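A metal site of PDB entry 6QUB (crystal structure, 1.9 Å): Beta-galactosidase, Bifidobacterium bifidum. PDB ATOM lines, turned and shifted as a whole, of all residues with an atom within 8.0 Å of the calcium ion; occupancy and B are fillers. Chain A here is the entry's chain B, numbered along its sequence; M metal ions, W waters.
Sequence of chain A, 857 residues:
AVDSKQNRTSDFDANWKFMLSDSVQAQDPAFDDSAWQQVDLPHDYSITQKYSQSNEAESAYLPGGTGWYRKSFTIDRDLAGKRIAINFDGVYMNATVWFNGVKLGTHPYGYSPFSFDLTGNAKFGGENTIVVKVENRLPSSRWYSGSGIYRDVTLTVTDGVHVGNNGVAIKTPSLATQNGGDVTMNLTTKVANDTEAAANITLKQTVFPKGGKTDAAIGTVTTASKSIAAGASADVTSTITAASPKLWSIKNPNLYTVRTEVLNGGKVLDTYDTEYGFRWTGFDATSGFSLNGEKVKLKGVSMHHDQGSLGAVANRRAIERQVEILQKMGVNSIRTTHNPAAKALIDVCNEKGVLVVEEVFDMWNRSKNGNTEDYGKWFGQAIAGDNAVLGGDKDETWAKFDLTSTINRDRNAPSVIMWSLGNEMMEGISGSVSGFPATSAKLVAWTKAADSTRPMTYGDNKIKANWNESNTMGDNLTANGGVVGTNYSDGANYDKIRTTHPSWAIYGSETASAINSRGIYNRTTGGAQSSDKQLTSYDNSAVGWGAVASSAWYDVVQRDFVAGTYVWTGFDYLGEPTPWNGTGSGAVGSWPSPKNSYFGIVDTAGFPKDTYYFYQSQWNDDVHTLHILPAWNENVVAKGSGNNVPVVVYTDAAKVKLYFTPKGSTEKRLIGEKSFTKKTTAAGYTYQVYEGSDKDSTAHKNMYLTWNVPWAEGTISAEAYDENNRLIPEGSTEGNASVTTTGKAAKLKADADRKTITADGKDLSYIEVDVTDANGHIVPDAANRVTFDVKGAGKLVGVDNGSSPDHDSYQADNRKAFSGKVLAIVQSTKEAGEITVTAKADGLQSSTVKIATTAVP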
ATOM      1  N   GLU A  56     -12.882  21.630  16.443  1.00  0.00           N
ATOM      2  CA  GLU A  56     -14.071  22.315  15.949  1.00  0.00           C
ATOM      3  C   GLU A  56     -13.787  23.079  14.657  1.00  0.00           C
ATOM      4  O   GLU A  56     -12.776  23.780  14.536  1.00  0.00           O
ATOM      5  CB  GLU A  56     -14.629  23.272  17.007  1.00  0.00           C
ATOM      6  CG  GLU A  56     -15.017  22.564  18.297  1.00  0.00           C
ATOM      7  CD  GLU A  56     -15.819  23.450  19.250  1.00  0.00           C
ATOM      8  OE1 GLU A  56     -15.969  24.657  18.957  1.00  0.00           O
ATOM      9  OE2 GLU A  56     -16.311  22.938  20.281  1.00  0.00           O
ATOM     10  N   ALA A  57     -14.714  22.965  13.701  1.00  0.00           N
ATOM     11  CA  ALA A  57     -14.550  23.599  12.394  1.00  0.00           C
ATOM     12  C   ALA A  57     -14.401  25.108  12.525  1.00  0.00           C
ATOM     13  O   ALA A  57     -13.603  25.717  11.798  1.00  0.00           O
ATOM     14  CB  ALA A  57     -15.727  23.250  11.488  1.00  0.00           C
ATOM     15  N   GLU A  58     -15.165  25.728  13.426  1.00  0.00           N
ATOM     16  CA  GLU A  58     -15.181  27.188  13.511  1.00  0.00           C
ATOM     17  C   GLU A  58     -13.809  27.752  13.869  1.00  0.00           C
ATOM     18  O   GLU A  58     -13.499  28.887  13.488  1.00  0.00           O
ATOM     19  CB  GLU A  58     -16.216  27.652  14.527  1.00  0.00           C
ATOM     20  CG  GLU A  58     -15.906  27.252  15.941  1.00  0.00           C
ATOM     21  CD  GLU A  58     -16.856  27.878  16.950  1.00  0.00           C
ATOM     22  OE1 GLU A  58     -17.813  28.570  16.538  1.00  0.00           O
ATOM     23  OE2 GLU A  58     -16.638  27.651  18.147  1.00  0.00           O
ATOM     24  N   SER A  59     -12.981  26.985  14.577  1.00  0.00           N
ATOM     25  CA  SER A  59     -11.622  27.373  14.915  1.00  0.00           C
ATOM     26  C   SER A  59     -10.590  26.543  14.148  1.00  0.00           C
ATOM     27  O   SER A  59      -9.497  26.274  14.650  1.00  0.00           O
ATOM     28  CB  SER A  59     -11.390  27.282  16.423  1.00  0.00           C
ATOM     29  OG  SER A  59     -11.873  26.047  16.929  1.00  0.00           O
ATOM     30  N   LEU A 138      -9.774  25.420  24.611  1.00  0.00           N
ATOM     31  CA  LEU A 138     -10.880  25.493  23.666  1.00  0.00           C
ATOM     32  C   LEU A 138     -12.134  24.980  24.359  1.00  0.00           C
ATOM     33  O   LEU A 138     -12.043  24.181  25.286  1.00  0.00           O
ATOM     34  CB  LEU A 138     -10.588  24.683  22.407  1.00  0.00           C
ATOM     35  CG  LEU A 138      -9.349  25.056  21.588  1.00  0.00           C
ATOM     36  CD1 LEU A 138      -9.504  24.494  20.175  1.00  0.00           C
ATOM     37  CD2 LEU A 138      -9.097  26.559  21.562  1.00  0.00           C
ATOM     38  N   PRO A 139     -13.316  25.456  23.929  1.00  0.00           N
ATOM     39  CA  PRO A 139     -13.567  26.425  22.859  1.00  0.00           C
ATOM     40  C   PRO A 139     -13.623  27.874  23.348  1.00  0.00           C
ATOM     41  O   PRO A 139     -14.274  28.158  24.357  1.00  0.00           O
ATOM     42  CB  PRO A 139     -14.921  25.981  22.309  1.00  0.00           C
ATOM     43  CG  PRO A 139     -15.634  25.444  23.513  1.00  0.00           C
ATOM     44  CD  PRO A 139     -14.578  24.885  24.455  1.00  0.00           C
ATOM     45  N   SER A 140     -12.959  28.791  22.638  1.00  0.00           N
ATOM     46  CA  SER A 140     -12.887  30.175  23.090  1.00  0.00           C
ATOM     47  C   SER A 140     -13.124  31.175  21.963  1.00  0.00           C
ATOM     48  O   SER A 140     -12.985  32.382  22.200  1.00  0.00           O
ATOM     49  CB  SER A 140     -11.525  30.455  23.716  1.00  0.00           C
ATOM     50  OG  SER A 140     -10.500  30.443  22.722  1.00  0.00           O
ATOM     51  N   SER A 141     -13.496  30.734  20.767  1.00  0.00           N
ATOM     52  CA  SER A 141     -13.527  31.644  19.635  1.00  0.00           C
ATOM     53  C   SER A 141     -14.463  31.109  18.557  1.00  0.00           C
ATOM     54  O   SER A 141     -14.572  29.901  18.381  1.00  0.00           O
ATOM     55  CB  SER A 141     -12.111  31.815  19.062  1.00  0.00           C
ATOM     56  OG  SER A 141     -12.069  32.848  18.091  1.00  0.00           O
ATOM     57  N   ARG A 142     -15.151  32.035  17.877  1.00  0.00           N
ATOM     58  CA  ARG A 142     -15.930  31.708  16.693  1.00  0.00           C
ATOM     59  C   ARG A 142     -15.075  31.639  15.433  1.00  0.00           C
ATOM     60  O   ARG A 142     -15.603  31.319  14.357  1.00  0.00           O
ATOM     61  CB  ARG A 142     -17.042  32.742  16.493  1.00  0.00           C
ATOM     62  CG  ARG A 142     -18.078  32.765  17.602  1.00  0.00           C
ATOM     63  CD  ARG A 142     -19.257  33.678  17.247  1.00  0.00           C
ATOM     64  NE  ARG A 142     -18.829  35.060  16.988  1.00  0.00           N
ATOM     65  CZ  ARG A 142     -18.772  35.621  15.782  1.00  0.00           C
ATOM     66  NH1 ARG A 142     -19.116  34.929  14.707  1.00  0.00           N
ATOM     67  NH2 ARG A 142     -18.380  36.873  15.662  1.00  0.00           N
ATOM     68  N   LYS A 368     -20.742  32.937  23.371  1.00  0.00           N
ATOM     69  CA  LYS A 368     -21.402  32.644  22.106  1.00  0.00           C
ATOM     70  C   LYS A 368     -21.124  31.223  21.640  1.00  0.00           C
ATOM     71  O   LYS A 368     -20.045  30.672  21.875  1.00  0.00           O
ATOM     72  CB  LYS A 368     -20.951  33.615  21.006  1.00  0.00           C
ATOM     73  CG  LYS A 368     -21.385  35.051  21.205  1.00  0.00           C
ATOM     74  CD  LYS A 368     -20.897  35.881  20.032  1.00  0.00           C
ATOM     75  CE  LYS A 368     -21.531  37.245  20.002  1.00  0.00           C
ATOM     76  NZ  LYS A 368     -21.244  37.958  18.712  1.00  0.00           N
ATOM     77  N   ASN A 369     -22.099  30.632  20.937  1.00  0.00           N
ATOM     78  CA  ASN A 369     -21.888  29.415  20.151  1.00  0.00           C
ATOM     79  C   ASN A 369     -21.337  28.261  20.985  1.00  0.00           C
ATOM     80  O   ASN A 369     -20.590  27.421  20.472  1.00  0.00           O
ATOM     81  CB  ASN A 369     -20.944  29.678  18.978  1.00  0.00           C
ATOM     82  CG  ASN A 369     -21.525  30.625  17.955  1.00  0.00           C
ATOM     83  OD1 ASN A 369     -22.541  31.278  18.194  1.00  0.00           O
ATOM     84  ND2 ASN A 369     -20.866  30.723  16.808  1.00  0.00           N
ATOM     85  N   GLY A 370     -21.667  28.211  22.275  1.00  0.00           N
ATOM     86  CA  GLY A 370     -21.129  27.181  23.134  1.00  0.00           C
ATOM     87  C   GLY A 370     -19.655  27.306  23.439  1.00  0.00           C
ATOM     88  O   GLY A 370     -19.043  26.350  23.908  1.00  0.00           O
ATOM     89  N   ASN A 371     -19.060  28.482  23.191  1.00  0.00           N
ATOM     90  CA  ASN A 371     -17.634  28.692  23.437  1.00  0.00           C
ATOM     91  C   ASN A 371     -17.457  29.138  24.890  1.00  0.00           C
ATOM     92  O   ASN A 371     -17.262  30.309  25.204  1.00  0.00           O
ATOM     93  CB  ASN A 371     -17.062  29.710  22.447  1.00  0.00           C
ATOM     94  CG  ASN A 371     -17.084  29.182  21.013  1.00  0.00           C
ATOM     95  OD1 ASN A 371     -16.975  27.981  20.779  1.00  0.00           O
ATOM     96  ND2 ASN A 371     -17.214  30.084  20.039  1.00  0.00           N
ATOM     97  N   THR A 372     -17.519  28.146  25.787  1.00  0.00           N
ATOM     98  CA  THR A 372     -17.587  28.422  27.225  1.00  0.00           C
ATOM     99  C   THR A 372     -16.313  29.062  27.750  1.00  0.00           C
ATOM    100  O   THR A 372     -16.342  29.650  28.846  1.00  0.00           O
ATOM    101  CB  THR A 372     -17.873  27.135  28.014  1.00  0.00           C
ATOM    102  OG1 THR A 372     -16.858  26.153  27.760  1.00  0.00           O
ATOM    103  CG2 THR A 372     -19.228  26.558  27.612  1.00  0.00           C
ATOM    104  N   ASP A 374     -14.671  31.428  25.967  1.00  0.00           N
ATOM    105  CA  ASP A 374     -14.416  32.715  25.319  1.00  0.00           C
ATOM    106  C   ASP A 374     -14.451  33.833  26.354  1.00  0.00           C
ATOM    107  O   ASP A 374     -14.612  33.610  27.562  1.00  0.00           O
ATOM    108  CB  ASP A 374     -15.385  32.946  24.158  1.00  0.00           C
ATOM    109  CG  ASP A 374     -16.824  33.242  24.577  1.00  0.00           C
ATOM    110  OD1 ASP A 374     -17.113  33.572  25.757  1.00  0.00           O
ATOM    111  OD2 ASP A 374     -17.697  33.171  23.684  1.00  0.00           O
ATOM    112  N   GLY A 582     -18.943  24.569  11.776  1.00  0.00           N
ATOM    113  CA  GLY A 582     -19.322  23.678  12.840  1.00  0.00           C
ATOM    114  C   GLY A 582     -18.925  24.278  14.173  1.00  0.00           C
ATOM    115  O   GLY A 582     -17.731  24.416  14.471  1.00  0.00           O
ATOM    116  N   THR A 583     -19.922  24.637  14.974  1.00  0.00           N
ATOM    117  CA  THR A 583     -19.643  25.211  16.278  1.00  0.00           C
ATOM    118  C   THR A 583     -19.389  24.153  17.351  1.00  0.00           C
ATOM    119  O   THR A 583     -19.012  24.509  18.467  1.00  0.00           O
ATOM    120  CB  THR A 583     -20.795  26.143  16.687  1.00  0.00           C
ATOM    121  OG1 THR A 583     -22.023  25.408  16.674  1.00  0.00           O
ATOM    122  CG2 THR A 583     -20.897  27.315  15.708  1.00  0.00           C
ATOM    123  N   GLY A 584     -19.592  22.876  17.027  1.00  0.00           N
ATOM    124  CA  GLY A 584     -19.197  21.784  17.884  1.00  0.00           C
ATOM    125  C   GLY A 584     -18.053  20.985  17.273  1.00  0.00           C
ATOM    126  O   GLY A 584     -17.369  21.425  16.341  1.00  0.00           O
ATOM    127  N   SER A 585     -17.864  19.776  17.803  1.00  0.00           N
ATOM    128  CA  SER A 585     -16.791  18.918  17.325  1.00  0.00           C
ATOM    129  C   SER A 585     -17.251  18.091  16.126  1.00  0.00           C
ATOM    130  O   SER A 585     -18.436  17.992  15.816  1.00  0.00           O
ATOM    131  CB  SER A 585     -16.301  18.016  18.460  1.00  0.00           C
ATOM    132  OG  SER A 585     -17.243  16.989  18.719  1.00  0.00           O
HETATM  133 CA    CA M   1     -18.001  26.335  19.664  1.00  0.00          CA
HETATM  134  O   HOH W   1     -18.374  24.791  21.333  1.00  0.00           O
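Of the 19 residues printed, 5 come within 4 Å of the calcium ion. The nearest printed residue that does not touch the calcium ion is Pro 139 (4.1 Å).
Water W1 lies within hydrogen-bond range of OE2 of Glu 56 (3.0 Å) and O of Gly 370 (3.1 Å).
The calcium ion is bound by the side-chain amide oxygen of Asn 371, water W1, the backbone carbonyl oxygen of Thr 583, the side-chain carboxylate of Glu 58 and the side-chain carboxylate of Glu 56. The calcium ion has five donor atoms within binding distance. Slightly farther from the calcium ion lies O of Asn 369 (2.9 Å).
The backbone carbonyl oxygen (O) of Ser 141 sits at hydrogen-bond distance from the side-chain amide nitrogen (ND2) of Asn 371 (3.1 Å). The backbone carbonyl oxygen (O) of Lys 368 lies close to the side-chain amide nitrogen (ND2) of Asn 371 (3.4 Å). N of Glu 58 lies within hydrogen-bond range of O of Gly 582 (3.1 Å). The backbone carbonyl oxygen (O) of Glu 56 lies within hydrogen-bond range of the side-chain hydroxyl (OG) of Ser 59, 3.4 Å away.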
